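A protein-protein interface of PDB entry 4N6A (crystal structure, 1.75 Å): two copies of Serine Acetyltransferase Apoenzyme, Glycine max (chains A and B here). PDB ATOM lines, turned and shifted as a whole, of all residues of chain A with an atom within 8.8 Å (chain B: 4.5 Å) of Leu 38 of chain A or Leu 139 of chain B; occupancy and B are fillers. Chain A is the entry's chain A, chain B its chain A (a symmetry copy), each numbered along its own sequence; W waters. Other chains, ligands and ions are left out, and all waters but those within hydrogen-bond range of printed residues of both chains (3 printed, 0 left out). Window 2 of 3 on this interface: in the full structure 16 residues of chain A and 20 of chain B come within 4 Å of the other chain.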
ATOM      1  N   ALA A  28     -11.527   1.627  -4.712  1.00  0.00           N
ATOM      2  CA  ALA A  28     -12.943   1.985  -4.647  1.00  0.00           C
ATOM      3  C   ALA A  28     -13.706   1.013  -3.752  1.00  0.00           C
ATOM      4  O   ALA A  28     -14.613   1.403  -2.995  1.00  0.00           O
ATOM      5  CB  ALA A  28     -13.557   2.014  -6.063  1.00  0.00           C
ATOM      6  N   ASP A  31     -13.085   1.821  -0.155  1.00  0.00           N
ATOM      7  CA  ASP A  31     -13.824   3.026   0.214  1.00  0.00           C
ATOM      8  C   ASP A  31     -15.317   2.730   0.346  1.00  0.00           C
ATOM      9  O   ASP A  31     -15.981   3.244   1.247  1.00  0.00           O
ATOM     10  CB  ASP A  31     -13.611   4.151  -0.810  1.00  0.00           C
ATOM     11  CG  ASP A  31     -12.273   4.863  -0.635  1.00  0.00           C
ATOM     12  OD1 ASP A  31     -11.528   4.542   0.315  1.00  0.00           O
ATOM     13  OD2 ASP A  31     -11.972   5.767  -1.447  1.00  0.00           O
ATOM     14  N   ALA A  32     -15.843   1.902  -0.547  1.00  0.00           N
ATOM     15  CA  ALA A  32     -17.278   1.579  -0.504  1.00  0.00           C
ATOM     16  C   ALA A  32     -17.613   0.794   0.766  1.00  0.00           C
ATOM     17  O   ALA A  32     -18.664   1.000   1.393  1.00  0.00           O
ATOM     18  CB  ALA A  32     -17.682   0.786  -1.745  1.00  0.00           C
ATOM     19  N   GLU A  33     -16.712  -0.107   1.148  1.00  0.00           N
ATOM     20  CA  GLU A  33     -16.909  -0.906   2.354  1.00  0.00           C
ATOM     21  C   GLU A  33     -16.825  -0.051   3.618  1.00  0.00           C
ATOM     22  O   GLU A  33     -17.505  -0.335   4.607  1.00  0.00           O
ATOM     23  CB  GLU A  33     -15.876  -2.047   2.417  1.00  0.00           C
ATOM     24  CG  GLU A  33     -16.115  -3.093   1.331  1.00  0.00           C
ATOM     25  CD  GLU A  33     -14.933  -4.022   1.111  1.00  0.00           C
ATOM     26  OE1 GLU A  33     -13.852  -3.772   1.686  1.00  0.00           O
ATOM     27  OE2 GLU A  33     -15.087  -4.997   0.348  1.00  0.00           O
ATOM     28  N   SER A  34     -15.995   0.986   3.595  1.00  0.00           N
ATOM     29  CA  SER A  34     -15.784   1.777   4.807  1.00  0.00           C
ATOM     30  C   SER A  34     -16.789   2.936   4.928  1.00  0.00           C
ATOM     31  O   SER A  34     -17.038   3.424   6.029  1.00  0.00           O
ATOM     32  CB  SER A  34     -14.359   2.334   4.860  1.00  0.00           C
ATOM     33  OG  SER A  34     -14.190   3.380   3.919  1.00  0.00           O
ATOM     34  N   GLU A  35     -17.355   3.375   3.809  1.00  0.00           N
ATOM     35  CA  GLU A  35     -18.247   4.559   3.826  1.00  0.00           C
ATOM     36  C   GLU A  35     -19.581   4.307   3.123  1.00  0.00           C
ATOM     37  O   GLU A  35     -19.714   4.477   1.911  1.00  0.00           O
ATOM     38  CB  GLU A  35     -17.566   5.755   3.171  1.00  0.00           C
ATOM     39  CG  GLU A  35     -18.388   7.050   3.267  1.00  0.00           C
ATOM     40  CD  GLU A  35     -18.979   7.240   4.663  1.00  0.00           C
ATOM     41  OE1 GLU A  35     -18.224   7.564   5.615  1.00  0.00           O
ATOM     42  OE2 GLU A  35     -20.198   7.032   4.817  1.00  0.00           O
ATOM     43  N   PRO A  36     -20.590   3.938   3.898  1.00  0.00           N
ATOM     44  CA  PRO A  36     -21.861   3.586   3.267  1.00  0.00           C
ATOM     45  C   PRO A  36     -22.529   4.737   2.550  1.00  0.00           C
ATOM     46  O   PRO A  36     -23.325   4.468   1.645  1.00  0.00           O
ATOM     47  CB  PRO A  36     -22.714   3.091   4.448  1.00  0.00           C
ATOM     48  CG  PRO A  36     -22.024   3.550   5.667  1.00  0.00           C
ATOM     49  CD  PRO A  36     -20.571   3.633   5.335  1.00  0.00           C
ATOM     50  N   ALA A  37     -22.208   5.987   2.897  1.00  0.00           N
ATOM     51  CA  ALA A  37     -22.792   7.127   2.195  1.00  0.00           C
ATOM     52  C   ALA A  37     -22.322   7.201   0.751  1.00  0.00           C
ATOM     53  O   ALA A  37     -23.005   7.783  -0.077  1.00  0.00           O
ATOM     54  CB  ALA A  37     -22.466   8.445   2.906  1.00  0.00           C
ATOM     55  N   LEU A  38     -21.155   6.625   0.459  1.00  0.00           N
ATOM     56  CA  LEU A  38     -20.563   6.692  -0.878  1.00  0.00           C
ATOM     57  C   LEU A  38     -20.595   5.362  -1.644  1.00  0.00           C
ATOM     58  O   LEU A  38     -20.219   5.327  -2.821  1.00  0.00           O
ATOM     59  CB  LEU A  38     -19.102   7.161  -0.779  1.00  0.00           C
ATOM     60  CG  LEU A  38     -18.903   8.587  -0.260  1.00  0.00           C
ATOM     61  CD1 LEU A  38     -17.421   8.856  -0.116  1.00  0.00           C
ATOM     62  CD2 LEU A  38     -19.539   9.604  -1.223  1.00  0.00           C
ATOM     63  N   ALA A  39     -21.039   4.297  -0.985  1.00  0.00           N
ATOM     64  CA  ALA A  39     -20.961   2.945  -1.570  1.00  0.00           C
ATOM     65  C   ALA A  39     -21.680   2.820  -2.921  1.00  0.00           C
ATOM     66  O   ALA A  39     -21.139   2.227  -3.859  1.00  0.00           O
ATOM     67  CB  ALA A  39     -21.519   1.913  -0.593  1.00  0.00           C
ATOM     68  N   SER A  40     -22.903   3.347  -3.024  1.00  0.00           N
ATOM     69  CA  SER A  40     -23.658   3.178  -4.272  1.00  0.00           C
ATOM     70  C   SER A  40     -23.042   3.947  -5.430  1.00  0.00           C
ATOM     71  O   SER A  40     -23.020   3.471  -6.560  1.00  0.00           O
ATOM     72  CB  SER A  40     -25.116   3.604  -4.079  1.00  0.00           C
ATOM     73  OG  SER A  40     -25.700   2.719  -3.130  1.00  0.00           O
ATOM     74  N   TYR A  41     -22.565   5.144  -5.129  1.00  0.00           N
ATOM     75  CA  TYR A  41     -21.913   5.993  -6.118  1.00  0.00           C
ATOM     76  C   TYR A  41     -20.602   5.360  -6.599  1.00  0.00           C
ATOM     77  O   TYR A  41     -20.291   5.366  -7.786  1.00  0.00           O
ATOM     78  CB  TYR A  41     -21.696   7.367  -5.493  1.00  0.00           C
ATOM     79  CG  TYR A  41     -20.540   8.164  -6.016  1.00  0.00           C
ATOM     80  CD1 TYR A  41     -20.630   8.821  -7.234  1.00  0.00           C
ATOM     81  CD2 TYR A  41     -19.366   8.291  -5.275  1.00  0.00           C
ATOM     82  CE1 TYR A  41     -19.581   9.573  -7.721  1.00  0.00           C
ATOM     83  CE2 TYR A  41     -18.306   9.052  -5.746  1.00  0.00           C
ATOM     84  CZ  TYR A  41     -18.420   9.687  -6.968  1.00  0.00           C
ATOM     85  OH  TYR A  41     -17.369  10.441  -7.442  1.00  0.00           O
ATOM     86  N   LEU A  42     -19.854   4.766  -5.679  1.00  0.00           N
ATOM     87  CA  LEU A  42     -18.631   4.061  -6.072  1.00  0.00           C
ATOM     88  C   LEU A  42     -18.980   2.820  -6.907  1.00  0.00           C
ATOM     89  O   LEU A  42     -18.274   2.483  -7.854  1.00  0.00           O
ATOM     90  CB  LEU A  42     -17.817   3.659  -4.837  1.00  0.00           C
ATOM     91  CG  LEU A  42     -17.240   4.862  -4.088  1.00  0.00           C
ATOM     92  CD1 LEU A  42     -16.692   4.457  -2.721  1.00  0.00           C
ATOM     93  CD2 LEU A  42     -16.147   5.519  -4.937  1.00  0.00           C
ATOM     94  N   TYR A  43     -20.063   2.130  -6.545  1.00  0.00           N
ATOM     95  CA  TYR A  43     -20.500   0.990  -7.342  1.00  0.00           C
ATOM     96  C   TYR A  43     -20.924   1.412  -8.756  1.00  0.00           C
ATOM     97  O   TYR A  43     -20.489   0.822  -9.751  1.00  0.00           O
ATOM     98  CB  TYR A  43     -21.667   0.255  -6.650  1.00  0.00           C
ATOM     99  CG  TYR A  43     -22.298  -0.769  -7.556  1.00  0.00           C
ATOM    100  CD1 TYR A  43     -21.688  -2.008  -7.749  1.00  0.00           C
ATOM    101  CD2 TYR A  43     -23.493  -0.495  -8.229  1.00  0.00           C
ATOM    102  CE1 TYR A  43     -22.246  -2.954  -8.589  1.00  0.00           C
ATOM    103  CE2 TYR A  43     -24.056  -1.439  -9.077  1.00  0.00           C
ATOM    104  CZ  TYR A  43     -23.424  -2.662  -9.243  1.00  0.00           C
ATOM    105  OH  TYR A  43     -23.968  -3.613 -10.071  1.00  0.00           O
ATOM    106  N   SER A  44     -21.764   2.433  -8.858  1.00  0.00           N
ATOM    107  CA  SER A  44     -22.301   2.801 -10.169  1.00  0.00           C
ATOM    108  C   SER A  44     -21.217   3.413 -11.065  1.00  0.00           C
ATOM    109  O   SER A  44     -21.223   3.201 -12.269  1.00  0.00           O
ATOM    110  CB  SER A  44     -23.465   3.775 -10.029  1.00  0.00           C
ATOM    111  OG  SER A  44     -23.009   4.990  -9.473  1.00  0.00           O
ATOM    112  N   THR A  45     -20.297   4.169 -10.474  1.00  0.00           N
ATOM    113  CA  THR A  45     -19.237   4.800 -11.247  1.00  0.00           C
ATOM    114  C   THR A  45     -18.073   3.861 -11.594  1.00  0.00           C
ATOM    115  O   THR A  45     -17.605   3.848 -12.734  1.00  0.00           O
ATOM    116  CB  THR A  45     -18.707   6.032 -10.498  1.00  0.00           C
ATOM    117  OG1 THR A  45     -19.812   6.880 -10.167  1.00  0.00           O
ATOM    118  CG2 THR A  45     -17.748   6.818 -11.367  1.00  0.00           C
ATOM    119  N   ILE A  46     -17.614   3.076 -10.623  1.00  0.00           N
ATOM    120  CA  ILE A  46     -16.415   2.271 -10.809  1.00  0.00           C
ATOM    121  C   ILE A  46     -16.666   0.771 -10.782  1.00  0.00           C
ATOM    122  O   ILE A  46     -16.375   0.082 -11.759  1.00  0.00           O
ATOM    123  CB  ILE A  46     -15.352   2.621  -9.735  1.00  0.00           C
ATOM    124  CG1 ILE A  46     -14.862   4.057  -9.960  1.00  0.00           C
ATOM    125  CG2 ILE A  46     -14.168   1.635  -9.793  1.00  0.00           C
ATOM    126  CD1 ILE A  46     -13.880   4.576  -8.914  1.00  0.00           C
ATOM    127  N   LEU A  47     -17.188   0.253  -9.671  1.00  0.00           N
ATOM    128  CA  LEU A  47     -17.165  -1.201  -9.442  1.00  0.00           C
ATOM    129  C   LEU A  47     -18.071  -1.979 -10.403  1.00  0.00           C
ATOM    130  O   LEU A  47     -17.839  -3.162 -10.660  1.00  0.00           O
ATOM    131  CB  LEU A  47     -17.565  -1.505  -7.999  1.00  0.00           C
ATOM    132  CG  LEU A  47     -16.639  -0.886  -6.944  1.00  0.00           C
ATOM    133  CD1 LEU A  47     -17.150  -1.170  -5.529  1.00  0.00           C
ATOM    134  CD2 LEU A  47     -15.203  -1.376  -7.120  1.00  0.00           C
ATOM    135  N   HIS A 111      -8.868   8.185  -6.245  1.00  0.00           N
ATOM    136  CA  HIS A 111      -9.241   9.503  -5.736  1.00  0.00           C
ATOM    137  C   HIS A 111      -8.968  10.558  -6.796  1.00  0.00           C
ATOM    138  O   HIS A 111      -9.724  11.516  -6.937  1.00  0.00           O
ATOM    139  CB  HIS A 111      -8.511   9.810  -4.429  1.00  0.00           C
ATOM    140  CG  HIS A 111      -8.989   8.987  -3.271  1.00  0.00           C
ATOM    141  ND1 HIS A 111      -8.336   8.957  -2.057  1.00  0.00           N
ATOM    142  CD2 HIS A 111     -10.068   8.176  -3.139  1.00  0.00           C
ATOM    143  CE1 HIS A 111      -8.984   8.155  -1.230  1.00  0.00           C
ATOM    144  NE2 HIS A 111     -10.042   7.672  -1.862  1.00  0.00           N
ATOM    145  N   LEU A 114     -11.826  10.167  -9.366  1.00  0.00           N
ATOM    146  CA  LEU A 114     -13.113  10.667  -8.884  1.00  0.00           C
ATOM    147  C   LEU A 114     -13.133  12.144  -8.488  1.00  0.00           C
ATOM    148  O   LEU A 114     -14.137  12.831  -8.719  1.00  0.00           O
ATOM    149  CB  LEU A 114     -13.575   9.847  -7.684  1.00  0.00           C
ATOM    150  CG  LEU A 114     -13.885   8.366  -7.905  1.00  0.00           C
ATOM    151  CD1 LEU A 114     -13.915   7.680  -6.555  1.00  0.00           C
ATOM    152  CD2 LEU A 114     -15.204   8.180  -8.631  1.00  0.00           C
ATOM    153  N   ASN A 115     -12.050  12.626  -7.876  1.00  0.00           N
ATOM    154  CA  ASN A 115     -12.100  13.907  -7.177  1.00  0.00           C
ATOM    155  C   ASN A 115     -11.189  14.994  -7.727  1.00  0.00           C
ATOM    156  O   ASN A 115     -11.358  16.154  -7.378  1.00  0.00           O
ATOM    157  CB  ASN A 115     -11.746  13.736  -5.699  1.00  0.00           C
ATOM    158  CG  ASN A 115     -12.710  12.837  -4.956  1.00  0.00           C
ATOM    159  OD1 ASN A 115     -13.898  12.776  -5.278  1.00  0.00           O
ATOM    160  ND2 ASN A 115     -12.206  12.151  -3.936  1.00  0.00           N
ATOM    161  N   THR B  68     -25.073  12.949  -5.892  1.00  0.00           N
ATOM    162  CA  THR B  68     -24.389  11.978  -5.051  1.00  0.00           C
ATOM    163  C   THR B  68     -24.874  12.058  -3.606  1.00  0.00           C
ATOM    164  O   THR B  68     -25.017  11.048  -2.941  1.00  0.00           O
ATOM    165  CB  THR B  68     -22.866  12.212  -5.103  1.00  0.00           C
ATOM    166  OG1 THR B  68     -22.425  12.135  -6.462  1.00  0.00           O
ATOM    167  CG2 THR B  68     -22.095  11.206  -4.249  1.00  0.00           C
ATOM    168  N   LEU B  77     -26.097  15.125   8.514  1.00  0.00           N
ATOM    169  CA  LEU B  77     -24.662  15.108   8.801  1.00  0.00           C
ATOM    170  C   LEU B  77     -24.229  16.354   9.568  1.00  0.00           C
ATOM    171  O   LEU B  77     -23.539  16.277  10.608  1.00  0.00           O
ATOM    172  CB  LEU B  77     -23.870  15.006   7.503  1.00  0.00           C
ATOM    173  CG  LEU B  77     -22.352  15.082   7.666  1.00  0.00           C
ATOM    174  CD1 LEU B  77     -21.814  13.757   8.181  1.00  0.00           C
ATOM    175  CD2 LEU B  77     -21.690  15.458   6.356  1.00  0.00           C
ATOM    176  N   LEU B 131     -14.874  14.864  10.349  1.00  0.00           N
ATOM    177  CA  LEU B 131     -14.974  13.568   9.669  1.00  0.00           C
ATOM    178  C   LEU B 131     -13.590  12.969   9.442  1.00  0.00           C
ATOM    179  O   LEU B 131     -13.376  11.783   9.677  1.00  0.00           O
ATOM    180  CB  LEU B 131     -15.716  13.713   8.340  1.00  0.00           C
ATOM    181  CG  LEU B 131     -17.209  14.021   8.443  1.00  0.00           C
ATOM    182  CD1 LEU B 131     -17.753  14.430   7.081  1.00  0.00           C
ATOM    183  CD2 LEU B 131     -17.960  12.796   8.962  1.00  0.00           C
ATOM    184  N   ARG B 136     -13.289   9.104   8.746  1.00  0.00           N
ATOM    185  CA  ARG B 136     -14.209   9.051   7.619  1.00  0.00           C
ATOM    186  C   ARG B 136     -13.647   9.950   6.520  1.00  0.00           C
ATOM    187  O   ARG B 136     -14.269  10.931   6.113  1.00  0.00           O
ATOM    188  CB  ARG B 136     -15.626   9.488   8.023  1.00  0.00           C
ATOM    189  CG  ARG B 136     -16.373   8.485   8.911  1.00  0.00           C
ATOM    190  CD  ARG B 136     -17.804   8.941   9.216  1.00  0.00           C
ATOM    191  NE  ARG B 136     -18.768   8.563   8.173  1.00  0.00           N
ATOM    192  CZ  ARG B 136     -20.067   8.859   8.225  1.00  0.00           C
ATOM    193  NH1 ARG B 136     -20.544   9.547   9.258  1.00  0.00           N
ATOM    194  NH2 ARG B 136     -20.894   8.467   7.256  1.00  0.00           N
ATOM    195  N   ARG B 137     -12.458   9.602   6.039  1.00  0.00           N
ATOM    196  CA  ARG B 137     -11.773  10.456   5.083  1.00  0.00           C
ATOM    197  C   ARG B 137     -12.383  10.481   3.675  1.00  0.00           C
ATOM    198  O   ARG B 137     -12.416  11.543   3.067  1.00  0.00           O
ATOM    199  CB  ARG B 137     -10.296  10.060   5.015  1.00  0.00           C
ATOM    200  CG  ARG B 137      -9.583  10.311   6.333  1.00  0.00           C
ATOM    201  CD  ARG B 137      -8.092  10.074   6.222  1.00  0.00           C
ATOM    202  NE  ARG B 137      -7.425  10.419   7.475  1.00  0.00           N
ATOM    203  CZ  ARG B 137      -6.111  10.370   7.650  1.00  0.00           C
ATOM    204  NH1 ARG B 137      -5.323  10.001   6.649  1.00  0.00           N
ATOM    205  NH2 ARG B 137      -5.588  10.698   8.823  1.00  0.00           N
ATOM    206  N   PRO B 138     -12.863   9.332   3.142  1.00  0.00           N
ATOM    207  CA  PRO B 138     -13.537   9.462   1.845  1.00  0.00           C
ATOM    208  C   PRO B 138     -14.707  10.437   1.880  1.00  0.00           C
ATOM    209  O   PRO B 138     -14.865  11.238   0.961  1.00  0.00           O
ATOM    210  CB  PRO B 138     -14.028   8.034   1.561  1.00  0.00           C
ATOM    211  CG  PRO B 138     -12.998   7.170   2.240  1.00  0.00           C
ATOM    212  CD  PRO B 138     -12.654   7.915   3.505  1.00  0.00           C
ATOM    213  N   LEU B 139     -15.511  10.384   2.936  1.00  0.00           N
ATOM    214  CA  LEU B 139     -16.625  11.317   3.063  1.00  0.00           C
ATOM    215  C   LEU B 139     -16.125  12.749   3.323  1.00  0.00           C
ATOM    216  O   LEU B 139     -16.703  13.714   2.823  1.00  0.00           O
ATOM    217  CB  LEU B 139     -17.573  10.880   4.182  1.00  0.00           C
ATOM    218  CG  LEU B 139     -18.832  11.732   4.346  1.00  0.00           C
ATOM    219  CD1 LEU B 139     -19.673  11.693   3.073  1.00  0.00           C
ATOM    220  CD2 LEU B 139     -19.644  11.285   5.561  1.00  0.00           C
ATOM    221  N   ALA B 140     -15.065  12.888   4.110  1.00  0.00           N
ATOM    222  CA  ALA B 140     -14.479  14.212   4.339  1.00  0.00           C
ATOM    223  C   ALA B 140     -14.067  14.829   3.016  1.00  0.00           C
ATOM    224  O   ALA B 140     -14.286  16.011   2.783  1.00  0.00           O
ATOM    225  CB  ALA B 140     -13.262  14.133   5.276  1.00  0.00           C
ATOM    226  N   LEU B 141     -13.469  14.016   2.149  1.00  0.00           N
ATOM    227  CA  LEU B 141     -13.007  14.499   0.857  1.00  0.00           C
ATOM    228  C   LEU B 141     -14.171  14.778  -0.091  1.00  0.00           C
ATOM    229  O   LEU B 141     -14.108  15.712  -0.893  1.00  0.00           O
ATOM    230  CB  LEU B 141     -12.037  13.497   0.235  1.00  0.00           C
ATOM    231  CG  LEU B 141     -10.733  13.350   1.034  1.00  0.00           C
ATOM    232  CD1 LEU B 141      -9.891  12.213   0.485  1.00  0.00           C
ATOM    233  CD2 LEU B 141      -9.971  14.675   1.014  1.00  0.00           C
ATOM    234  N   ALA B 142     -15.229  13.977  -0.011  1.00  0.00           N
ATOM    235  CA  ALA B 142     -16.397  14.234  -0.848  1.00  0.00           C
ATOM    236  C   ALA B 142     -17.038  15.560  -0.445  1.00  0.00           C
ATOM    237  O   ALA B 142     -17.486  16.338  -1.292  1.00  0.00           O
ATOM    238  CB  ALA B 142     -17.418  13.087  -0.745  1.00  0.00           C
ATOM    239  N   LEU B 143     -17.081  15.818   0.854  1.00  0.00           N
ATOM    240  CA  LEU B 143     -17.671  17.058   1.344  1.00  0.00           C
ATOM    241  C   LEU B 143     -16.786  18.225   0.918  1.00  0.00           C
ATOM    242  O   LEU B 143     -17.271  19.240   0.440  1.00  0.00           O
ATOM    243  CB  LEU B 143     -17.824  17.021   2.862  1.00  0.00           C
ATOM    244  CG  LEU B 143     -18.327  18.299   3.542  1.00  0.00           C
ATOM    245  CD1 LEU B 143     -19.596  18.816   2.871  1.00  0.00           C
ATOM    246  CD2 LEU B 143     -18.571  18.062   5.036  1.00  0.00           C
HETATM  247  O   HOH W   1     -25.323   9.286  -0.122  1.00  0.00           O
HETATM  248  O   HOH W   2     -15.688   8.076   4.886  1.00  0.00           O
HETATM  249  O   HOH W   3     -14.039  10.798  -1.781  1.00  0.00           O
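Asp 31 of chain A touches Pro 138 of chain B.
OE1 of Glu 35 of chain A touches CB of Leu 139 of chain B (3.7 Å).
Leu 38 of chain A touches Pro 138 of chain B (CD1 to O, 3.7 Å).
Leu 139 of chain B touches Leu 38 of chain A (N to CD1, 3.9 Å).
Tyr 41 of chain A touches Thr 68 of chain B.
The backbone carbonyl oxygen (O) of Tyr 41 of chain A is in hydrogen-bond range of the side-chain hydroxyl (OG1) of Thr 45 of chain A, 2.9 Å away.
The backbone NH (N) of Ala 37 of chain A lies within hydrogen-bond range of the side-chain carboxylate (OE2) of Glu 35 of chain A (3.0 Å).
The side-chain carboxylate (OD2) of Asp 31 of chain A sits at hydrogen-bond distance from a ring nitrogen (NE2) of His 111 of chain A, 2.7 Å away.
O of Asp 31 of chain A lies within hydrogen-bond range of OG of Ser 34 of chain A, at 3.2 Å.
The backbone carbonyl oxygen (O) of Tyr 41 of chain A sits at hydrogen-bond distance from the side-chain hydroxyl (OG) of Ser 44 of chain A, at 3.2 Å.
The backbone carbonyl oxygen (O) of Leu 131 of chain B sits at hydrogen-bond distance from the backbone NH (N) of Arg 136 of chain B (2.8 Å).
No position is printed for both chains.
Of the 6 pairs that touch across the chains among the printed residues, none has its exchanged pair printed and touching as well.
Of the 11 printed residues of chain B, 4 touch a printed residue of chain A.
Hydrophobic or aromatic side chains of chain B within 4 Å of the printed part of chain A: Pro 138 and Leu 139.
Of the 21 printed residues of chain A, 4 touch a printed residue of chain B.
Hydrophobic or aromatic side chains of chain A that line the printed part of chain B: Leu 38 and Tyr 41.
Among the printed residues, Asp or Glu carboxylates within 4 Å of a Lys or Arg side-chain nitrogen of the other chain: Glu 35 of chain A with Arg 136 of chain B (2.8 Å).
Leu 38 of chain A touches two residues of chain B.
Of chain A, only Glu 35 and Leu 38 come within 4 Å of Leu 139 of chain B.
Of the printed residues of chain A, Pro 138 of chain B touches Asp 31 (3.6 Å) and Leu 38 (3.7 Å).
No residue of chain A comes within 4 Å of Ala 140 of chain B.
Of the printed residues of chain A, Arg 136 of chain B touches Glu 35 (2.8 Å).
Of the printed residues of chain A, Thr 68 of chain B touches Tyr 41 (3.8 Å).
Of the printed residues of chain B, Tyr 41 of chain A touches Thr 68.
Of the printed residues of chain B, Asp 31 of chain A touches Pro 138 (3.6 Å).
Printed residues of chain B within 4 Å of Glu 35 of chain A: Arg 136 (2.8 Å) and Leu 139 (3.7 Å).
The guanidinium group of Arg 136 of chain B is in salt-bridge range of the side-chain carboxylate of Glu 35 of chain A, 2.8 Å away.
Water W2 lies within hydrogen-bond range of OE1 of Glu 35 of chain A, N of Leu 139 of chain B and O of Arg 136 of chain B.
Water W1 bridges the backbone carbonyl oxygen of Ala 37 of chain A and the backbone carbonyl oxygen of Thr 68 of chain B.
Water W3 lies within hydrogen-bond range of O of Pro 138 of chain B and ND2 of Asn 115 of chain A.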
